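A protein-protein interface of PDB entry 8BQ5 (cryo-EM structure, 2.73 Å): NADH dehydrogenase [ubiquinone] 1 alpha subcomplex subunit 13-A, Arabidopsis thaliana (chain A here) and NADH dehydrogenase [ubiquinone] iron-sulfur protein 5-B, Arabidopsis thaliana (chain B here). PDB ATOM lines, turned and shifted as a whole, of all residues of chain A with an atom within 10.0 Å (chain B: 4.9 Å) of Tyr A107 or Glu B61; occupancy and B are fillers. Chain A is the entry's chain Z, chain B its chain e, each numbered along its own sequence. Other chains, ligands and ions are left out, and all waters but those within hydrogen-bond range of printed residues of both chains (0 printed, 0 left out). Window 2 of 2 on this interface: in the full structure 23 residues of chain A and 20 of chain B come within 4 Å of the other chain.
The side-chain hydroxyl (OH) of Tyr A107 sits at hydrogen-bond distance from the side-chain carboxylate (OE2) of Glu B61 (2.9 Å). The backbone carbonyl oxygen (O) of Lys A113 lies within hydrogen-bond range of the side-chain amino group (NZ) of Lys B64, at 3.1 Å.
NE1 of Trp A118 sits at hydrogen-bond distance from OE1 of Glu A108. The side-chain carboxylate (OE2) of Glu A108 is in hydrogen-bond range of the backbone NH (N) of Gly A121 (3.1 Å). NE of Arg B63 lies within salt-bridge range of OE2 of Glu B60 (3.2 Å).
Among the printed residues, merely in contact across the chains: Met A112 with Ile B57 (3.5 Å), Glu A108 with Ile B57 (3.6 Å), Trp A118 with Ile B57 (3.6 Å), Met A112 with Glu B60 (3.7 Å), Val A111 with Glu B60 (3.7 Å), Val A115 with Glu B60 (3.7 Å), Tyr A104 with Ile B57 (3.9 Å) and Val A111 with Ile B57 (3.9 Å).
Tyr A107 touches just one residue of chain B: Glu B61. Printed residues of chain B within 4 Å of Met A112: Ile B57 and Glu B60. Glu B61 touches just one residue of chain A: Tyr A107 (2.9 Å). Of the printed residues of chain A, Lys B64 touches Lys A113 (3.1 Å). No residue of chain A comes within 4 Å of Leu B65. The nearest residue of chain B that does not touch Tyr A107 is Ile B57 (4.4 Å). The nearest printed residue of chain B that does not touch Met A112 is Glu B61 (5.5 Å).
Among the printed residues, 10 pairs touch across the chains.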
ATOM      1  N   SER A  99     -17.803  22.049 -14.681  1.00  0.00           N
ATOM      2  CA  SER A  99     -17.148  22.058 -13.375  1.00  0.00           C
ATOM      3  C   SER A  99     -17.682  23.188 -12.493  1.00  0.00           C
ATOM      4  O   SER A  99     -17.992  22.974 -11.310  1.00  0.00           O
ATOM      5  CB  SER A  99     -15.633  22.175 -13.547  1.00  0.00           C
ATOM      6  OG  SER A  99     -15.200  23.512 -13.378  1.00  0.00           O
ATOM      7  N   GLU A 100     -17.823  24.391 -13.059  1.00  0.00           N
ATOM      8  CA  GLU A 100     -18.350  25.510 -12.283  1.00  0.00           C
ATOM      9  C   GLU A 100     -19.779  25.244 -11.824  1.00  0.00           C
ATOM     10  O   GLU A 100     -20.168  25.622 -10.711  1.00  0.00           O
ATOM     11  CB  GLU A 100     -18.285  26.797 -13.106  1.00  0.00           C
ATOM     12  CG  GLU A 100     -17.018  27.606 -12.901  1.00  0.00           C
ATOM     13  CD  GLU A 100     -16.596  27.666 -11.446  1.00  0.00           C
ATOM     14  OE1 GLU A 100     -17.146  28.504 -10.700  1.00  0.00           O
ATOM     15  OE2 GLU A 100     -15.710  26.880 -11.050  1.00  0.00           O
ATOM     16  N   TRP A 101     -20.578  24.601 -12.674  1.00  0.00           N
ATOM     17  CA  TRP A 101     -21.957  24.303 -12.320  1.00  0.00           C
ATOM     18  C   TRP A 101     -22.026  23.280 -11.198  1.00  0.00           C
ATOM     19  O   TRP A 101     -22.891  23.373 -10.324  1.00  0.00           O
ATOM     20  CB  TRP A 101     -22.718  23.813 -13.548  1.00  0.00           C
ATOM     21  CG  TRP A 101     -24.172  23.639 -13.293  1.00  0.00           C
ATOM     22  CD1 TRP A 101     -24.885  22.481 -13.382  1.00  0.00           C
ATOM     23  CD2 TRP A 101     -25.099  24.651 -12.887  1.00  0.00           C
ATOM     24  NE1 TRP A 101     -26.200  22.711 -13.064  1.00  0.00           N
ATOM     25  CE2 TRP A 101     -26.357  24.036 -12.757  1.00  0.00           C
ATOM     26  CE3 TRP A 101     -24.987  26.021 -12.627  1.00  0.00           C
ATOM     27  CZ2 TRP A 101     -27.495  24.740 -12.376  1.00  0.00           C
ATOM     28  CZ3 TRP A 101     -26.118  26.718 -12.250  1.00  0.00           C
ATOM     29  CH2 TRP A 101     -27.356  26.077 -12.127  1.00  0.00           C
ATOM     30  N   LYS A 102     -21.127  22.293 -11.206  1.00  0.00           N
ATOM     31  CA  LYS A 102     -21.057  21.369 -10.077  1.00  0.00           C
ATOM     32  C   LYS A 102     -20.709  22.104  -8.788  1.00  0.00           C
ATOM     33  O   LYS A 102     -21.303  21.840  -7.732  1.00  0.00           O
ATOM     34  CB  LYS A 102     -20.040  20.266 -10.361  1.00  0.00           C
ATOM     35  CG  LYS A 102     -20.640  19.047 -11.031  1.00  0.00           C
ATOM     36  CD  LYS A 102     -19.582  18.010 -11.356  1.00  0.00           C
ATOM     37  CE  LYS A 102     -19.485  17.788 -12.855  1.00  0.00           C
ATOM     38  NZ  LYS A 102     -19.412  16.345 -13.203  1.00  0.00           N
ATOM     39  N   LYS A 103     -19.753  23.034  -8.856  1.00  0.00           N
ATOM     40  CA  LYS A 103     -19.405  23.798  -7.659  1.00  0.00           C
ATOM     41  C   LYS A 103     -20.599  24.600  -7.143  1.00  0.00           C
ATOM     42  O   LYS A 103     -20.875  24.612  -5.935  1.00  0.00           O
ATOM     43  CB  LYS A 103     -18.216  24.718  -7.941  1.00  0.00           C
ATOM     44  CG  LYS A 103     -17.030  24.014  -8.580  1.00  0.00           C
ATOM     45  CD  LYS A 103     -15.773  24.148  -7.741  1.00  0.00           C
ATOM     46  CE  LYS A 103     -14.526  23.868  -8.567  1.00  0.00           C
ATOM     47  NZ  LYS A 103     -14.352  24.849  -9.675  1.00  0.00           N
ATOM     48  N   TYR A 104     -21.331  25.261  -8.043  1.00  0.00           N
ATOM     49  CA  TYR A 104     -22.479  26.047  -7.599  1.00  0.00           C
ATOM     50  C   TYR A 104     -23.598  25.150  -7.082  1.00  0.00           C
ATOM     51  O   TYR A 104     -24.317  25.524  -6.149  1.00  0.00           O
ATOM     52  CB  TYR A 104     -22.991  26.948  -8.725  1.00  0.00           C
ATOM     53  CG  TYR A 104     -24.314  27.610  -8.397  1.00  0.00           C
ATOM     54  CD1 TYR A 104     -24.357  28.776  -7.643  1.00  0.00           C
ATOM     55  CD2 TYR A 104     -25.515  27.072  -8.838  1.00  0.00           C
ATOM     56  CE1 TYR A 104     -25.558  29.383  -7.335  1.00  0.00           C
ATOM     57  CE2 TYR A 104     -26.720  27.672  -8.534  1.00  0.00           C
ATOM     58  CZ  TYR A 104     -26.736  28.827  -7.783  1.00  0.00           C
ATOM     59  OH  TYR A 104     -27.934  29.430  -7.480  1.00  0.00           O
ATOM     60  N   LEU A 105     -23.773  23.968  -7.678  1.00  0.00           N
ATOM     61  CA  LEU A 105     -24.786  23.040  -7.189  1.00  0.00           C
ATOM     62  C   LEU A 105     -24.473  22.581  -5.772  1.00  0.00           C
ATOM     63  O   LEU A 105     -25.376  22.481  -4.936  1.00  0.00           O
ATOM     64  CB  LEU A 105     -24.909  21.837  -8.124  1.00  0.00           C
ATOM     65  CG  LEU A 105     -25.722  22.047  -9.403  1.00  0.00           C
ATOM     66  CD1 LEU A 105     -25.683  20.802 -10.274  1.00  0.00           C
ATOM     67  CD2 LEU A 105     -27.153  22.423  -9.066  1.00  0.00           C
ATOM     68  N   GLU A 106     -23.201  22.301  -5.480  1.00  0.00           N
ATOM     69  CA  GLU A 106     -22.860  21.895  -4.119  1.00  0.00           C
ATOM     70  C   GLU A 106     -22.991  23.064  -3.145  1.00  0.00           C
ATOM     71  O   GLU A 106     -23.413  22.880  -1.995  1.00  0.00           O
ATOM     72  CB  GLU A 106     -21.459  21.282  -4.074  1.00  0.00           C
ATOM     73  CG  GLU A 106     -20.308  22.258  -3.930  1.00  0.00           C
ATOM     74  CD  GLU A 106     -18.973  21.608  -4.225  1.00  0.00           C
ATOM     75  OE1 GLU A 106     -17.928  22.181  -3.850  1.00  0.00           O
ATOM     76  OE2 GLU A 106     -18.972  20.515  -4.828  1.00  0.00           O
ATOM     77  N   TYR A 107     -22.666  24.281  -3.595  1.00  0.00           N
ATOM     78  CA  TYR A 107     -22.877  25.453  -2.750  1.00  0.00           C
ATOM     79  C   TYR A 107     -24.356  25.618  -2.412  1.00  0.00           C
ATOM     80  O   TYR A 107     -24.717  25.900  -1.264  1.00  0.00           O
ATOM     81  CB  TYR A 107     -22.326  26.702  -3.444  1.00  0.00           C
ATOM     82  CG  TYR A 107     -22.874  28.022  -2.941  1.00  0.00           C
ATOM     83  CD1 TYR A 107     -24.064  28.542  -3.440  1.00  0.00           C
ATOM     84  CD2 TYR A 107     -22.196  28.757  -1.979  1.00  0.00           C
ATOM     85  CE1 TYR A 107     -24.565  29.743  -2.987  1.00  0.00           C
ATOM     86  CE2 TYR A 107     -22.690  29.966  -1.522  1.00  0.00           C
ATOM     87  CZ  TYR A 107     -23.876  30.452  -2.031  1.00  0.00           C
ATOM     88  OH  TYR A 107     -24.380  31.652  -1.585  1.00  0.00           O
ATOM     89  N   GLU A 108     -25.226  25.451  -3.410  1.00  0.00           N
ATOM     90  CA  GLU A 108     -26.662  25.557  -3.177  1.00  0.00           C
ATOM     91  C   GLU A 108     -27.156  24.440  -2.267  1.00  0.00           C
ATOM     92  O   GLU A 108     -28.014  24.668  -1.407  1.00  0.00           O
ATOM     93  CB  GLU A 108     -27.414  25.536  -4.507  1.00  0.00           C
ATOM     94  CG  GLU A 108     -28.877  25.914  -4.385  1.00  0.00           C
ATOM     95  CD  GLU A 108     -29.764  25.164  -5.357  1.00  0.00           C
ATOM     96  OE1 GLU A 108     -30.877  24.767  -4.958  1.00  0.00           O
ATOM     97  OE2 GLU A 108     -29.351  24.976  -6.521  1.00  0.00           O
ATOM     98  N   ALA A 109     -26.630  23.227  -2.449  1.00  0.00           N
ATOM     99  CA  ALA A 109     -27.001  22.117  -1.579  1.00  0.00           C
ATOM    100  C   ALA A 109     -26.635  22.410  -0.132  1.00  0.00           C
ATOM    101  O   ALA A 109     -27.364  22.031   0.790  1.00  0.00           O
ATOM    102  CB  ALA A 109     -26.327  20.831  -2.055  1.00  0.00           C
ATOM    103  N   ASP A 110     -25.499  23.076   0.087  1.00  0.00           N
ATOM    104  CA  ASP A 110     -25.102  23.413   1.452  1.00  0.00           C
ATOM    105  C   ASP A 110     -25.948  24.548   2.024  1.00  0.00           C
ATOM    106  O   ASP A 110     -26.393  24.480   3.175  1.00  0.00           O
ATOM    107  CB  ASP A 110     -23.620  23.779   1.495  1.00  0.00           C
ATOM    108  CG  ASP A 110     -23.035  23.646   2.882  1.00  0.00           C
ATOM    109  OD1 ASP A 110     -22.805  22.499   3.323  1.00  0.00           O
ATOM    110  OD2 ASP A 110     -22.813  24.686   3.537  1.00  0.00           O
ATOM    111  N   VAL A 111     -26.169  25.607   1.241  1.00  0.00           N
ATOM    112  CA  VAL A 111     -26.866  26.783   1.764  1.00  0.00           C
ATOM    113  C   VAL A 111     -28.338  26.475   2.000  1.00  0.00           C
ATOM    114  O   VAL A 111     -28.901  26.824   3.046  1.00  0.00           O
ATOM    115  CB  VAL A 111     -26.680  27.984   0.816  1.00  0.00           C
ATOM    116  CG1 VAL A 111     -27.805  28.988   0.993  1.00  0.00           C
ATOM    117  CG2 VAL A 111     -25.339  28.652   1.063  1.00  0.00           C
ATOM    118  N   MET A 112     -28.982  25.810   1.046  1.00  0.00           N
ATOM    119  CA  MET A 112     -30.388  25.459   1.169  1.00  0.00           C
ATOM    120  C   MET A 112     -30.612  24.211   2.009  1.00  0.00           C
ATOM    121  O   MET A 112     -31.691  23.616   1.938  1.00  0.00           O
ATOM    122  CB  MET A 112     -31.015  25.280  -0.215  1.00  0.00           C
ATOM    123  CG  MET A 112     -30.907  26.506  -1.105  1.00  0.00           C
ATOM    124  SD  MET A 112     -30.973  28.053  -0.179  1.00  0.00           S
ATOM    125  CE  MET A 112     -32.740  28.331  -0.111  1.00  0.00           C
ATOM    126  N   LYS A 113     -29.620  23.792   2.790  1.00  0.00           N
ATOM    127  CA  LYS A 113     -29.851  22.730   3.755  1.00  0.00           C
ATOM    128  C   LYS A 113     -30.742  23.249   4.878  1.00  0.00           C
ATOM    129  O   LYS A 113     -30.633  24.409   5.291  1.00  0.00           O
ATOM    130  CB  LYS A 113     -28.526  22.214   4.312  1.00  0.00           C
ATOM    131  CG  LYS A 113     -28.681  20.979   5.171  1.00  0.00           C
ATOM    132  CD  LYS A 113     -27.379  20.235   5.337  1.00  0.00           C
ATOM    133  CE  LYS A 113     -27.515  19.136   6.378  1.00  0.00           C
ATOM    134  NZ  LYS A 113     -26.297  18.283   6.425  1.00  0.00           N
ATOM    135  N   VAL A 115     -34.003  23.604   4.461  1.00  0.00           N
ATOM    136  CA  VAL A 115     -35.086  24.350   3.832  1.00  0.00           C
ATOM    137  C   VAL A 115     -36.076  23.333   3.266  1.00  0.00           C
ATOM    138  O   VAL A 115     -35.792  22.702   2.237  1.00  0.00           O
ATOM    139  CB  VAL A 115     -34.577  25.302   2.742  1.00  0.00           C
ATOM    140  CG1 VAL A 115     -35.662  26.293   2.371  1.00  0.00           C
ATOM    141  CG2 VAL A 115     -33.341  26.045   3.222  1.00  0.00           C
ATOM    142  N   TRP A 118     -37.134  22.080  -0.842  1.00  0.00           N
ATOM    143  CA  TRP A 118     -36.224  22.588  -1.855  1.00  0.00           C
ATOM    144  C   TRP A 118     -35.756  21.473  -2.786  1.00  0.00           C
ATOM    145  O   TRP A 118     -35.814  20.283  -2.464  1.00  0.00           O
ATOM    146  CB  TRP A 118     -35.016  23.266  -1.211  1.00  0.00           C
ATOM    147  CG  TRP A 118     -34.315  24.219  -2.127  1.00  0.00           C
ATOM    148  CD1 TRP A 118     -33.091  24.046  -2.707  1.00  0.00           C
ATOM    149  CD2 TRP A 118     -34.793  25.492  -2.574  1.00  0.00           C
ATOM    150  NE1 TRP A 118     -32.779  25.131  -3.486  1.00  0.00           N
ATOM    151  CE2 TRP A 118     -33.807  26.035  -3.422  1.00  0.00           C
ATOM    152  CE3 TRP A 118     -35.960  26.228  -2.341  1.00  0.00           C
ATOM    153  CZ2 TRP A 118     -33.950  27.278  -4.035  1.00  0.00           C
ATOM    154  CZ3 TRP A 118     -36.099  27.461  -2.953  1.00  0.00           C
ATOM    155  CH2 TRP A 118     -35.100  27.973  -3.788  1.00  0.00           C
ATOM    156  N   VAL A 120     -32.378  20.939  -5.427  1.00  0.00           N
ATOM    157  CA  VAL A 120     -31.113  21.520  -5.855  1.00  0.00           C
ATOM    158  C   VAL A 120     -31.021  21.481  -7.375  1.00  0.00           C
ATOM    159  O   VAL A 120     -31.082  20.410  -7.992  1.00  0.00           O
ATOM    160  CB  VAL A 120     -29.935  20.784  -5.199  1.00  0.00           C
ATOM    161  CG1 VAL A 120     -28.616  21.270  -5.774  1.00  0.00           C
ATOM    162  CG2 VAL A 120     -29.966  20.986  -3.690  1.00  0.00           C
ATOM    163  N   GLY A 121     -30.865  22.653  -7.983  1.00  0.00           N
ATOM    164  CA  GLY A 121     -30.802  22.749  -9.434  1.00  0.00           C
ATOM    165  C   GLY A 121     -32.091  22.398 -10.146  1.00  0.00           C
ATOM    166  O   GLY A 121     -32.063  21.689 -11.159  1.00  0.00           O
ATOM    167  N   ILE B  57     -32.413  31.771  -2.492  1.00  0.00           N
ATOM    168  CA  ILE B  57     -31.125  31.244  -2.041  1.00  0.00           C
ATOM    169  C   ILE B  57     -30.334  32.331  -1.317  1.00  0.00           C
ATOM    170  O   ILE B  57     -29.770  32.108  -0.236  1.00  0.00           O
ATOM    171  CB  ILE B  57     -30.344  30.669  -3.236  1.00  0.00           C
ATOM    172  CG1 ILE B  57     -30.772  29.227  -3.499  1.00  0.00           C
ATOM    173  CG2 ILE B  57     -28.846  30.743  -2.992  1.00  0.00           C
ATOM    174  CD1 ILE B  57     -30.800  28.858  -4.958  1.00  0.00           C
ATOM    175  N   TYR B  58     -30.306  33.532  -1.901  1.00  0.00           N
ATOM    176  CA  TYR B  58     -29.624  34.666  -1.280  1.00  0.00           C
ATOM    177  C   TYR B  58     -30.227  35.004   0.079  1.00  0.00           C
ATOM    178  O   TYR B  58     -29.500  35.308   1.033  1.00  0.00           O
ATOM    179  CB  TYR B  58     -29.693  35.872  -2.219  1.00  0.00           C
ATOM    180  CG  TYR B  58     -29.564  37.227  -1.555  1.00  0.00           C
ATOM    181  CD1 TYR B  58     -28.324  37.828  -1.384  1.00  0.00           C
ATOM    182  CD2 TYR B  58     -30.688  37.911  -1.106  1.00  0.00           C
ATOM    183  CE1 TYR B  58     -28.209  39.070  -0.785  1.00  0.00           C
ATOM    184  CE2 TYR B  58     -30.582  39.146  -0.501  1.00  0.00           C
ATOM    185  CZ  TYR B  58     -29.344  39.722  -0.345  1.00  0.00           C
ATOM    186  OH  TYR B  58     -29.248  40.956   0.255  1.00  0.00           O
ATOM    187  N   LYS B  59     -31.558  34.976   0.177  1.00  0.00           N
ATOM    188  CA  LYS B  59     -32.233  35.291   1.431  1.00  0.00           C
ATOM    189  C   LYS B  59     -31.871  34.288   2.515  1.00  0.00           C
ATOM    190  O   LYS B  59     -31.612  34.664   3.664  1.00  0.00           O
ATOM    191  CB  LYS B  59     -33.747  35.314   1.221  1.00  0.00           C
ATOM    192  CG  LYS B  59     -34.500  36.119   2.269  1.00  0.00           C
ATOM    193  CD  LYS B  59     -35.934  36.424   1.852  1.00  0.00           C
ATOM    194  CE  LYS B  59     -36.102  36.471   0.343  1.00  0.00           C
ATOM    195  NZ  LYS B  59     -37.447  36.991  -0.027  1.00  0.00           N
ATOM    196  N   GLU B  60     -31.866  32.999   2.173  1.00  0.00           N
ATOM    197  CA  GLU B  60     -31.507  31.988   3.162  1.00  0.00           C
ATOM    198  C   GLU B  60     -30.054  32.134   3.596  1.00  0.00           C
ATOM    199  O   GLU B  60     -29.732  31.984   4.783  1.00  0.00           O
ATOM    200  CB  GLU B  60     -31.774  30.588   2.616  1.00  0.00           C
ATOM    201  CG  GLU B  60     -31.388  29.485   3.583  1.00  0.00           C
ATOM    202  CD  GLU B  60     -32.366  29.348   4.733  1.00  0.00           C
ATOM    203  OE1 GLU B  60     -33.586  29.493   4.507  1.00  0.00           O
ATOM    204  OE2 GLU B  60     -31.910  29.104   5.869  1.00  0.00           O
ATOM    205  N   GLU B  61     -29.161  32.431   2.650  1.00  0.00           N
ATOM    206  CA  GLU B  61     -27.764  32.648   3.012  1.00  0.00           C
ATOM    207  C   GLU B  61     -27.623  33.832   3.962  1.00  0.00           C
ATOM    208  O   GLU B  61     -26.905  33.750   4.966  1.00  0.00           O
ATOM    209  CB  GLU B  61     -26.924  32.861   1.755  1.00  0.00           C
ATOM    210  CG  GLU B  61     -25.428  32.795   1.987  1.00  0.00           C
ATOM    211  CD  GLU B  61     -24.653  33.566   0.941  1.00  0.00           C
ATOM    212  OE1 GLU B  61     -25.211  34.535   0.386  1.00  0.00           O
ATOM    213  OE2 GLU B  61     -23.493  33.198   0.662  1.00  0.00           O
ATOM    214  N   GLN B  62     -28.314  34.937   3.669  1.00  0.00           N
ATOM    215  CA  GLN B  62     -28.275  36.100   4.552  1.00  0.00           C
ATOM    216  C   GLN B  62     -28.848  35.787   5.927  1.00  0.00           C
ATOM    217  O   GLN B  62     -28.317  36.257   6.939  1.00  0.00           O
ATOM    218  CB  GLN B  62     -29.034  37.265   3.918  1.00  0.00           C
ATOM    219  CG  GLN B  62     -28.345  38.618   4.022  1.00  0.00           C
ATOM    220  CD  GLN B  62     -26.967  38.647   3.385  1.00  0.00           C
ATOM    221  OE1 GLN B  62     -26.640  37.817   2.536  1.00  0.00           O
ATOM    222  NE2 GLN B  62     -26.158  39.621   3.782  1.00  0.00           N
ATOM    223  N   ARG B  63     -29.934  35.014   5.983  1.00  0.00           N
ATOM    224  CA  ARG B  63     -30.518  34.640   7.267  1.00  0.00           C
ATOM    225  C   ARG B  63     -29.550  33.805   8.094  1.00  0.00           C
ATOM    226  O   ARG B  63     -29.420  34.016   9.306  1.00  0.00           O
ATOM    227  CB  ARG B  63     -31.826  33.880   7.046  1.00  0.00           C
ATOM    228  CG  ARG B  63     -32.601  33.618   8.320  1.00  0.00           C
ATOM    229  CD  ARG B  63     -33.703  32.594   8.112  1.00  0.00           C
ATOM    230  NE  ARG B  63     -33.195  31.272   7.764  1.00  0.00           N
ATOM    231  CZ  ARG B  63     -32.703  30.402   8.636  1.00  0.00           C
ATOM    232  NH1 ARG B  63     -32.557  30.712   9.915  1.00  0.00           N
ATOM    233  NH2 ARG B  63     -32.350  29.191   8.217  1.00  0.00           N
ATOM    234  N   LYS B  64     -28.852  32.860   7.460  1.00  0.00           N
ATOM    235  CA  LYS B  64     -27.930  31.978   8.166  1.00  0.00           C
ATOM    236  C   LYS B  64     -26.526  32.561   8.284  1.00  0.00           C
ATOM    237  O   LYS B  64     -25.555  31.805   8.420  1.00  0.00           O
ATOM    238  CB  LYS B  64     -27.877  30.611   7.482  1.00  0.00           C
ATOM    239  CG  LYS B  64     -29.135  29.774   7.649  1.00  0.00           C
ATOM    240  CD  LYS B  64     -28.971  28.402   7.009  1.00  0.00           C
ATOM    241  CE  LYS B  64     -29.736  27.332   7.776  1.00  0.00           C
ATOM    242  NZ  LYS B  64     -29.207  25.964   7.526  1.00  0.00           N
ATOM    243  N   LEU B  65     -26.389  33.881   8.233  1.00  0.00           N
ATOM    244  CA  LEU B  65     -25.082  34.508   8.368  1.00  0.00           C
ATOM    245  C   LEU B  65     -25.083  35.530   9.502  1.00  0.00           C
ATOM    246  O   LEU B  65     -25.660  36.608   9.378  1.00  0.00           O
ATOM    247  CB  LEU B  65     -24.669  35.180   7.060  1.00  0.00           C
ATOM    248  CG  LEU B  65     -23.314  35.886   7.100  1.00  0.00           C
ATOM    249  CD1 LEU B  65     -22.186  34.867   7.218  1.00  0.00           C
ATOM    250  CD2 LEU B  65     -23.127  36.777   5.884  1.00  0.00           C
